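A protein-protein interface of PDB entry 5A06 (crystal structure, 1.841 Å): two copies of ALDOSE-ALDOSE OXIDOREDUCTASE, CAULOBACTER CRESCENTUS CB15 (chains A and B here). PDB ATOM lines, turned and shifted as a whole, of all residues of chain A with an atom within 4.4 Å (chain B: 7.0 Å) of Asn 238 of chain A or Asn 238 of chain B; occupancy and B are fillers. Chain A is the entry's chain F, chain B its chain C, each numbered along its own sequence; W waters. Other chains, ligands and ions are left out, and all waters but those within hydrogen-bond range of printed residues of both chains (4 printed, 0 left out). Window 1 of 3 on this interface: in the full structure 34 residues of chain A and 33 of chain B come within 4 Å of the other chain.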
ATOM      1  N   VAL A 157     -17.908 -21.677 -10.613  1.00  0.00           N
ATOM      2  CA  VAL A 157     -16.856 -20.862 -10.018  1.00  0.00           C
ATOM      3  C   VAL A 157     -16.064 -21.758  -9.079  1.00  0.00           C
ATOM      4  O   VAL A 157     -16.616 -22.309  -8.113  1.00  0.00           O
ATOM      5  CB  VAL A 157     -17.419 -19.667  -9.238  1.00  0.00           C
ATOM      6  CG1 VAL A 157     -16.292 -18.902  -8.531  1.00  0.00           C
ATOM      7  CG2 VAL A 157     -18.192 -18.741 -10.169  1.00  0.00           C
ATOM      8  N   VAL A 158     -14.775 -21.914  -9.349  1.00  0.00           N
ATOM      9  CA  VAL A 158     -13.932 -22.718  -8.474  1.00  0.00           C
ATOM     10  C   VAL A 158     -12.899 -21.766  -7.868  1.00  0.00           C
ATOM     11  O   VAL A 158     -12.120 -21.143  -8.593  1.00  0.00           O
ATOM     12  CB  VAL A 158     -13.263 -23.883  -9.240  1.00  0.00           C
ATOM     13  CG1 VAL A 158     -12.252 -24.604  -8.358  1.00  0.00           C
ATOM     14  CG2 VAL A 158     -14.331 -24.868  -9.751  1.00  0.00           C
ATOM     15  N   THR A 159     -12.932 -21.614  -6.553  1.00  0.00           N
ATOM     16  CA  THR A 159     -12.107 -20.604  -5.901  1.00  0.00           C
ATOM     17  C   THR A 159     -11.550 -21.106  -4.569  1.00  0.00           C
ATOM     18  O   THR A 159     -12.257 -21.713  -3.763  1.00  0.00           O
ATOM     19  CB  THR A 159     -12.920 -19.294  -5.714  1.00  0.00           C
ATOM     20  OG1 THR A 159     -12.121 -18.315  -5.043  1.00  0.00           O
ATOM     21  CG2 THR A 159     -14.197 -19.537  -4.922  1.00  0.00           C
ATOM     22  N   ASN A 226     -14.494 -26.188   3.677  1.00  0.00           N
ATOM     23  CA  ASN A 226     -14.775 -26.048   2.253  1.00  0.00           C
ATOM     24  C   ASN A 226     -16.280 -26.032   2.040  1.00  0.00           C
ATOM     25  O   ASN A 226     -16.999 -26.706   2.775  1.00  0.00           O
ATOM     26  CB  ASN A 226     -14.138 -27.192   1.462  1.00  0.00           C
ATOM     27  CG  ASN A 226     -12.627 -27.232   1.622  1.00  0.00           C
ATOM     28  OD1 ASN A 226     -12.007 -26.198   1.862  1.00  0.00           O
ATOM     29  ND2 ASN A 226     -12.031 -28.419   1.500  1.00  0.00           N
ATOM     30  N   PHE A 227     -16.758 -25.274   1.060  1.00  0.00           N
ATOM     31  CA  PHE A 227     -18.204 -25.169   0.879  1.00  0.00           C
ATOM     32  C   PHE A 227     -18.653 -25.126  -0.592  1.00  0.00           C
ATOM     33  O   PHE A 227     -17.883 -24.765  -1.496  1.00  0.00           O
ATOM     34  CB  PHE A 227     -18.741 -23.943   1.656  1.00  0.00           C
ATOM     35  CG  PHE A 227     -18.018 -22.640   1.364  1.00  0.00           C
ATOM     36  CD1 PHE A 227     -16.833 -22.313   2.031  1.00  0.00           C
ATOM     37  CD2 PHE A 227     -18.550 -21.720   0.468  1.00  0.00           C
ATOM     38  CE1 PHE A 227     -16.179 -21.104   1.778  1.00  0.00           C
ATOM     39  CE2 PHE A 227     -17.917 -20.493   0.226  1.00  0.00           C
ATOM     40  CZ  PHE A 227     -16.723 -20.194   0.873  1.00  0.00           C
ATOM     41  N   GLN A 228     -19.907 -25.522  -0.824  1.00  0.00           N
ATOM     42  CA  GLN A 228     -20.518 -25.486  -2.148  1.00  0.00           C
ATOM     43  C   GLN A 228     -21.699 -24.529  -2.122  1.00  0.00           C
ATOM     44  O   GLN A 228     -22.436 -24.499  -1.131  1.00  0.00           O
ATOM     45  CB  GLN A 228     -21.011 -26.871  -2.582  1.00  0.00           C
ATOM     46  CG  GLN A 228     -20.021 -27.992  -2.408  1.00  0.00           C
ATOM     47  CD  GLN A 228     -20.569 -29.284  -2.977  1.00  0.00           C
ATOM     48  OE1 GLN A 228     -21.435 -29.915  -2.377  1.00  0.00           O
ATOM     49  NE2 GLN A 228     -20.083 -29.672  -4.157  1.00  0.00           N
ATOM     50  N   ALA A 237     -20.753 -22.989  -7.241  1.00  0.00           N
ATOM     51  CA  ALA A 237     -19.407 -22.661  -6.752  1.00  0.00           C
ATOM     52  C   ALA A 237     -18.867 -23.747  -5.829  1.00  0.00           C
ATOM     53  O   ALA A 237     -19.585 -24.257  -4.968  1.00  0.00           O
ATOM     54  CB  ALA A 237     -19.407 -21.317  -6.024  1.00  0.00           C
ATOM     55  N   ASN A 238     -17.592 -24.087  -6.020  1.00  0.00           N
ATOM     56  CA  ASN A 238     -16.849 -24.969  -5.137  1.00  0.00           C
ATOM     57  C   ASN A 238     -15.773 -24.097  -4.521  1.00  0.00           C
ATOM     58  O   ASN A 238     -14.964 -23.545  -5.265  1.00  0.00           O
ATOM     59  CB  ASN A 238     -16.190 -26.118  -5.905  1.00  0.00           C
ATOM     60  CG  ASN A 238     -16.942 -27.444  -5.791  1.00  0.00           C
ATOM     61  OD1 ASN A 238     -18.083 -27.516  -5.329  1.00  0.00           O
ATOM     62  ND2 ASN A 238     -16.297 -28.506  -6.263  1.00  0.00           N
ATOM     63  N   CYS A 239     -15.763 -23.961  -3.200  1.00  0.00           N
ATOM     64  CA  CYS A 239     -14.842 -23.039  -2.527  1.00  0.00           C
ATOM     65  C   CYS A 239     -14.002 -23.710  -1.449  1.00  0.00           C
ATOM     66  O   CYS A 239     -14.501 -24.551  -0.685  1.00  0.00           O
ATOM     67  CB  CYS A 239     -15.628 -21.883  -1.899  1.00  0.00           C
ATOM     68  SG  CYS A 239     -16.859 -21.109  -2.997  1.00  0.00           S
ATOM     69  N   VAL A 240     -12.738 -23.301  -1.362  1.00  0.00           N
ATOM     70  CA  VAL A 240     -11.837 -23.738  -0.297  1.00  0.00           C
ATOM     71  C   VAL A 240     -11.519 -22.559   0.620  1.00  0.00           C
ATOM     72  O   VAL A 240     -11.303 -21.437   0.137  1.00  0.00           O
ATOM     73  CB  VAL A 240     -10.519 -24.319  -0.868  1.00  0.00           C
ATOM     74  CG1 VAL A 240      -9.425 -24.386   0.211  1.00  0.00           C
ATOM     75  CG2 VAL A 240     -10.774 -25.690  -1.480  1.00  0.00           C
ATOM     76  N   THR B 156      -5.742 -30.483   1.035  1.00  0.00           N
ATOM     77  CA  THR B 156      -6.775 -30.287   0.016  1.00  0.00           C
ATOM     78  C   THR B 156      -6.424 -30.876  -1.353  1.00  0.00           C
ATOM     79  O   THR B 156      -5.271 -30.841  -1.800  1.00  0.00           O
ATOM     80  CB  THR B 156      -7.096 -28.782  -0.209  1.00  0.00           C
ATOM     81  OG1 THR B 156      -5.927 -28.108  -0.695  1.00  0.00           O
ATOM     82  CG2 THR B 156      -7.581 -28.112   1.068  1.00  0.00           C
ATOM     83  N   VAL B 157      -7.440 -31.415  -2.023  1.00  0.00           N
ATOM     84  CA  VAL B 157      -7.349 -31.728  -3.434  1.00  0.00           C
ATOM     85  C   VAL B 157      -8.468 -30.971  -4.133  1.00  0.00           C
ATOM     86  O   VAL B 157      -9.633 -31.137  -3.793  1.00  0.00           O
ATOM     87  CB  VAL B 157      -7.508 -33.222  -3.739  1.00  0.00           C
ATOM     88  CG1 VAL B 157      -7.518 -33.437  -5.256  1.00  0.00           C
ATOM     89  CG2 VAL B 157      -6.408 -34.035  -3.069  1.00  0.00           C
ATOM     90  N   VAL B 158      -8.120 -30.133  -5.091  1.00  0.00           N
ATOM     91  CA  VAL B 158      -9.135 -29.417  -5.869  1.00  0.00           C
ATOM     92  C   VAL B 158      -9.017 -29.827  -7.329  1.00  0.00           C
ATOM     93  O   VAL B 158      -7.974 -29.618  -7.963  1.00  0.00           O
ATOM     94  CB  VAL B 158      -8.986 -27.890  -5.720  1.00  0.00           C
ATOM     95  CG1 VAL B 158      -9.984 -27.137  -6.639  1.00  0.00           C
ATOM     96  CG2 VAL B 158      -9.173 -27.496  -4.273  1.00  0.00           C
ATOM     97  N   THR B 159     -10.076 -30.434  -7.868  1.00  0.00           N
ATOM     98  CA  THR B 159      -9.982 -31.036  -9.194  1.00  0.00           C
ATOM     99  C   THR B 159     -11.285 -30.871  -9.991  1.00  0.00           C
ATOM    100  O   THR B 159     -12.388 -31.056  -9.447  1.00  0.00           O
ATOM    101  CB  THR B 159      -9.587 -32.553  -9.085  1.00  0.00           C
ATOM    102  OG1 THR B 159      -9.499 -33.139 -10.385  1.00  0.00           O
ATOM    103  CG2 THR B 159     -10.588 -33.350  -8.219  1.00  0.00           C
ATOM    104  N   ASP B 160     -11.144 -30.494 -11.264  1.00  0.00           N
ATOM    105  CA  ASP B 160     -12.285 -30.199 -12.141  1.00  0.00           C
ATOM    106  C   ASP B 160     -12.143 -30.966 -13.447  1.00  0.00           C
ATOM    107  O   ASP B 160     -11.120 -30.859 -14.125  1.00  0.00           O
ATOM    108  CB  ASP B 160     -12.391 -28.696 -12.464  1.00  0.00           C
ATOM    109  CG  ASP B 160     -12.265 -27.812 -11.236  1.00  0.00           C
ATOM    110  OD1 ASP B 160     -12.724 -28.228 -10.161  1.00  0.00           O
ATOM    111  OD2 ASP B 160     -11.718 -26.684 -11.357  1.00  0.00           O
ATOM    112  N   SER B 190     -12.064 -36.889 -11.634  1.00  0.00           N
ATOM    113  CA  SER B 190     -11.879 -36.103 -10.417  1.00  0.00           C
ATOM    114  C   SER B 190     -11.866 -36.999  -9.182  1.00  0.00           C
ATOM    115  O   SER B 190     -11.015 -36.869  -8.294  1.00  0.00           O
ATOM    116  CB  SER B 190     -12.989 -35.054 -10.277  1.00  0.00           C
ATOM    117  OG  SER B 190     -12.907 -34.095 -11.313  1.00  0.00           O
ATOM    118  N   ALA B 194      -8.679 -37.810  -6.700  1.00  0.00           N
ATOM    119  CA  ALA B 194      -8.727 -37.527  -5.261  1.00  0.00           C
ATOM    120  C   ALA B 194      -8.277 -38.758  -4.466  1.00  0.00           C
ATOM    121  O   ALA B 194      -7.523 -38.653  -3.496  1.00  0.00           O
ATOM    122  CB  ALA B 194     -10.128 -37.092  -4.825  1.00  0.00           C
ATOM    123  N   VAL B 208     -23.877 -31.372  -4.939  1.00  0.00           N
ATOM    124  CA  VAL B 208     -24.897 -30.481  -5.486  1.00  0.00           C
ATOM    125  C   VAL B 208     -25.032 -30.748  -6.980  1.00  0.00           C
ATOM    126  O   VAL B 208     -24.028 -30.730  -7.694  1.00  0.00           O
ATOM    127  CB  VAL B 208     -24.532 -28.987  -5.285  1.00  0.00           C
ATOM    128  CG1 VAL B 208     -25.616 -28.087  -5.886  1.00  0.00           C
ATOM    129  CG2 VAL B 208     -24.341 -28.678  -3.827  1.00  0.00           C
ATOM    130  N   ASN B 226     -21.303 -31.399  -8.614  1.00  0.00           N
ATOM    131  CA  ASN B 226     -20.070 -31.127  -7.890  1.00  0.00           C
ATOM    132  C   ASN B 226     -20.098 -31.828  -6.538  1.00  0.00           C
ATOM    133  O   ASN B 226     -21.166 -31.992  -5.931  1.00  0.00           O
ATOM    134  CB  ASN B 226     -19.862 -29.615  -7.730  1.00  0.00           C
ATOM    135  CG  ASN B 226     -19.781 -28.888  -9.079  1.00  0.00           C
ATOM    136  OD1 ASN B 226     -19.371 -29.468 -10.081  1.00  0.00           O
ATOM    137  ND2 ASN B 226     -20.213 -27.620  -9.110  1.00  0.00           N
ATOM    138  N   PHE B 227     -18.940 -32.267  -6.061  1.00  0.00           N
ATOM    139  CA  PHE B 227     -18.936 -33.004  -4.805  1.00  0.00           C
ATOM    140  C   PHE B 227     -17.747 -32.689  -3.906  1.00  0.00           C
ATOM    141  O   PHE B 227     -16.727 -32.149  -4.351  1.00  0.00           O
ATOM    142  CB  PHE B 227     -19.029 -34.525  -5.070  1.00  0.00           C
ATOM    143  CG  PHE B 227     -18.021 -35.076  -6.075  1.00  0.00           C
ATOM    144  CD1 PHE B 227     -18.224 -34.949  -7.448  1.00  0.00           C
ATOM    145  CD2 PHE B 227     -16.921 -35.800  -5.634  1.00  0.00           C
ATOM    146  CE1 PHE B 227     -17.322 -35.488  -8.361  1.00  0.00           C
ATOM    147  CE2 PHE B 227     -16.014 -36.339  -6.535  1.00  0.00           C
ATOM    148  CZ  PHE B 227     -16.210 -36.178  -7.906  1.00  0.00           C
ATOM    149  N   GLN B 228     -17.926 -32.990  -2.626  1.00  0.00           N
ATOM    150  CA  GLN B 228     -16.903 -32.794  -1.602  1.00  0.00           C
ATOM    151  C   GLN B 228     -16.618 -34.133  -0.962  1.00  0.00           C
ATOM    152  O   GLN B 228     -17.543 -34.896  -0.705  1.00  0.00           O
ATOM    153  CB  GLN B 228     -17.364 -31.823  -0.523  1.00  0.00           C
ATOM    154  CG  GLN B 228     -17.839 -30.473  -1.020  1.00  0.00           C
ATOM    155  CD  GLN B 228     -18.114 -29.539   0.144  1.00  0.00           C
ATOM    156  OE1 GLN B 228     -19.073 -29.733   0.898  1.00  0.00           O
ATOM    157  NE2 GLN B 228     -17.243 -28.543   0.327  1.00  0.00           N
ATOM    158  N   LEU B 229     -15.354 -34.414  -0.701  1.00  0.00           N
ATOM    159  CA  LEU B 229     -14.970 -35.655  -0.033  1.00  0.00           C
ATOM    160  C   LEU B 229     -14.197 -35.333   1.233  1.00  0.00           C
ATOM    161  O   LEU B 229     -13.398 -34.395   1.238  1.00  0.00           O
ATOM    162  CB  LEU B 229     -14.113 -36.523  -0.964  1.00  0.00           C
ATOM    163  CG  LEU B 229     -14.688 -36.883  -2.343  1.00  0.00           C
ATOM    164  CD1 LEU B 229     -13.629 -37.520  -3.233  1.00  0.00           C
ATOM    165  CD2 LEU B 229     -15.882 -37.823  -2.204  1.00  0.00           C
ATOM    166  N   THR B 236      -9.203 -33.231   2.568  1.00  0.00           N
ATOM    167  CA  THR B 236     -10.455 -32.900   1.883  1.00  0.00           C
ATOM    168  C   THR B 236     -10.297 -32.819   0.353  1.00  0.00           C
ATOM    169  O   THR B 236      -9.216 -32.509  -0.162  1.00  0.00           O
ATOM    170  CB  THR B 236     -11.009 -31.554   2.378  1.00  0.00           C
ATOM    171  OG1 THR B 236     -10.065 -30.530   2.064  1.00  0.00           O
ATOM    172  CG2 THR B 236     -11.233 -31.583   3.880  1.00  0.00           C
ATOM    173  N   ALA B 237     -11.373 -33.088  -0.386  1.00  0.00           N
ATOM    174  CA  ALA B 237     -11.366 -32.826  -1.821  1.00  0.00           C
ATOM    175  C   ALA B 237     -12.616 -32.043  -2.240  1.00  0.00           C
ATOM    176  O   ALA B 237     -13.716 -32.317  -1.756  1.00  0.00           O
ATOM    177  CB  ALA B 237     -11.258 -34.139  -2.622  1.00  0.00           C
ATOM    178  N   ASN B 238     -12.419 -31.040  -3.091  1.00  0.00           N
ATOM    179  CA  ASN B 238     -13.493 -30.319  -3.789  1.00  0.00           C
ATOM    180  C   ASN B 238     -13.425 -30.680  -5.272  1.00  0.00           C
ATOM    181  O   ASN B 238     -12.392 -30.448  -5.924  1.00  0.00           O
ATOM    182  CB  ASN B 238     -13.348 -28.794  -3.647  1.00  0.00           C
ATOM    183  CG  ASN B 238     -14.190 -28.175  -2.508  1.00  0.00           C
ATOM    184  OD1 ASN B 238     -14.811 -28.856  -1.681  1.00  0.00           O
ATOM    185  ND2 ASN B 238     -14.186 -26.849  -2.469  1.00  0.00           N
ATOM    186  N   CYS B 239     -14.510 -31.229  -5.820  1.00  0.00           N
ATOM    187  CA  CYS B 239     -14.471 -31.780  -7.170  1.00  0.00           C
ATOM    188  C   CYS B 239     -15.600 -31.266  -8.052  1.00  0.00           C
ATOM    189  O   CYS B 239     -16.736 -31.148  -7.601  1.00  0.00           O
ATOM    190  CB  CYS B 239     -14.550 -33.305  -7.125  1.00  0.00           C
ATOM    191  SG  CYS B 239     -13.394 -34.113  -5.992  1.00  0.00           S
ATOM    192  N   VAL B 240     -15.272 -30.983  -9.311  1.00  0.00           N
ATOM    193  CA  VAL B 240     -16.248 -30.586 -10.332  1.00  0.00           C
ATOM    194  C   VAL B 240     -16.388 -31.683 -11.382  1.00  0.00           C
ATOM    195  O   VAL B 240     -15.392 -32.246 -11.830  1.00  0.00           O
ATOM    196  CB  VAL B 240     -15.830 -29.258 -11.023  1.00  0.00           C
ATOM    197  CG1 VAL B 240     -16.545 -29.064 -12.373  1.00  0.00           C
ATOM    198  CG2 VAL B 240     -16.081 -28.067 -10.082  1.00  0.00           C
ATOM    199  N   SER B 241     -17.634 -31.987 -11.743  1.00  0.00           N
ATOM    200  CA  SER B 241     -17.982 -32.881 -12.840  1.00  0.00           C
ATOM    201  C   SER B 241     -18.999 -32.145 -13.718  1.00  0.00           C
ATOM    202  O   SER B 241     -20.041 -31.725 -13.207  1.00  0.00           O
ATOM    203  CB  SER B 241     -18.578 -34.190 -12.293  1.00  0.00           C
ATOM    204  OG  SER B 241     -19.041 -35.035 -13.335  1.00  0.00           O
HETATM  205  O   HOH W   1     -13.950 -30.396   0.508  1.00  0.00           O
HETATM  206  O   HOH W   2     -20.596 -26.704  -6.241  1.00  0.00           O
HETATM  207  O   HOH W   3     -13.651 -28.171  -7.466  1.00  0.00           O
HETATM  208  O   HOH W   4     -12.569 -25.302  -4.540  1.00  0.00           O
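Water W2 lies within hydrogen-bond range of the side-chain amide oxygen (OD1) of Asn 238 of chain A (2.8 Å), the backbone carbonyl oxygen (O) of Ala 237 of chain A (2.9 Å) and the side-chain amide nitrogen (ND2) of Asn 226 of chain B (3.0 Å).
Water W1 lies within hydrogen-bond range of OD1 of Asn 238 of chain B (2.8 Å), ND2 of Asn 226 of chain A (2.9 Å) and O of Ala 237 of chain B (3.0 Å).
Water W3 lies within hydrogen-bond range of OD1 of Asp 160 of chain B (2.9 Å), ND2 of Asn 238 of chain A (2.9 Å) and O of Asn 238 of chain B (3.0 Å).
Water W4 lies within hydrogen-bond range of ND2 of Asn 238 of chain B (3.0 Å) and O of Asn 238 of chain A (3.1 Å).
O of Asn 226 of chain B sits at hydrogen-bond distance from NE2 of Gln 228 of chain A.
N of Phe 227 of chain B sits close to NE2 of Gln 228 of chain A, at 3.4 Å.
NE2 of Gln 228 of chain B sits at hydrogen-bond distance from O of Asn 226 of chain A, at 3.1 Å.
The side-chain amide nitrogen (NE2) of Gln 228 of chain B sits close to the backbone NH (N) of Phe 227 of chain A (3.4 Å).
The side-chain hydroxyl of Thr 236 of chain B lies within hydrogen-bond range of the side-chain amide nitrogen of Asn 226 of chain A, at 2.9 Å.
The side-chain amide nitrogen (ND2) of Asn 238 of chain B sits at hydrogen-bond distance from the backbone carbonyl oxygen (O) of Cys 239 of chain A (2.9 Å).
The side-chain amide nitrogen of Asn 238 of chain A lies within hydrogen-bond range of the backbone carbonyl oxygen of Cys 239 of chain B (3.0 Å).
Of the 18 printed residues of chain B, 10 touch a printed residue of chain A.
Hydrophobic or aromatic side chains of chain B that line the printed part of chain A: Val 158, Val 208 and Val 240.
Among the printed residues, no Asp or Glu carboxylate lies within 4 Å of a Lys or Arg side-chain nitrogen of the other chain.
The backbone carbonyl oxygen (O) of Thr 159 of chain B is in hydrogen-bond range of the backbone NH (N) of Val 240 of chain B, 2.9 Å away.
The backbone carbonyl oxygen (O) of Asn 226 of chain B is in hydrogen-bond range of the backbone NH (N) of Val 208 of chain B (3.0 Å).
The backbone NH (N) of Cys 239 of chain B is in hydrogen-bond range of the backbone carbonyl oxygen (O) of Phe 227 of chain B, 2.8 Å away.
N of Thr 159 of chain A lies within hydrogen-bond range of O of Asn 238 of chain A, at 3.1 Å.
N of Val 240 of chain A sits at hydrogen-bond distance from O of Thr 159 of chain A (2.9 Å).
N of Cys 239 of chain A sits at hydrogen-bond distance from O of Phe 227 of chain A (2.8 Å).
Asn 238 of chain A touches four residues of chain B.
Asn 238 of chain B touches four residues of chain A.
Of the printed residues of chain A, Gln 228 of chain B touches Asn 226, Phe 227 and Gln 228.
Of the printed residues of chain B, Gln 228 of chain A touches Val 208, Asn 226, Phe 227 and Gln 228.
Of the printed residues of chain B, Asn 226 of chain A touches Gln 228, Thr 236 and Asn 238.
Printed residues of chain B within 4 Å of Cys 239 of chain A: Asn 238 (2.9 Å).
The nearest printed residue of chain A that does not touch Asn 226 of chain B is Ala 237 of chain A (5.0 Å).
Among the printed residues, pairs that only touch across the chains: Gln 228 of chain A with Val 208 of chain B (3.5 Å), Gln 228 of chain A with Gln 228 of chain B (3.5 Å), Val 158 of chain A with Asp 160 of chain B (3.6 Å), Asn 226 of chain A with Asn 238 of chain B (3.6 Å), Asn 238 of chain A with Asn 226 of chain B (3.7 Å), Val 158 of chain A with Val 240 of chain B (3.7 Å), Val 240 of chain A with Val 158 of chain B (3.7 Å), Asn 238 of chain A with Asn 238 of chain B (3.7 Å), Val 240 of chain A with Asn 238 of chain B (3.7 Å), Val 158 of chain A with Val 158 of chain B (3.8 Å) and Asn 238 of chain A with Val 240 of chain B (3.9 Å).
Val 158 of chain A touches Val 240 of chain B, and with the chains exchanged Val 240 of chain A touches Val 158 of chain B.
Asn 226 of chain A touches Gln 228 of chain B, and with the chains exchanged Gln 228 of chain A touches Asn 226 of chain B.
Asn 226 of chain A touches Asn 238 of chain B, and with the chains exchanged Asn 238 of chain A touches Asn 226 of chain B.
Asn 238 of chain A touches Cys 239 of chain B, and with the chains exchanged Cys 239 of chain A touches Asn 238 of chain B.
Positions printed for both chains: 157, 158, 159, 226, 227, 228, 237, 238, 239 and 240.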
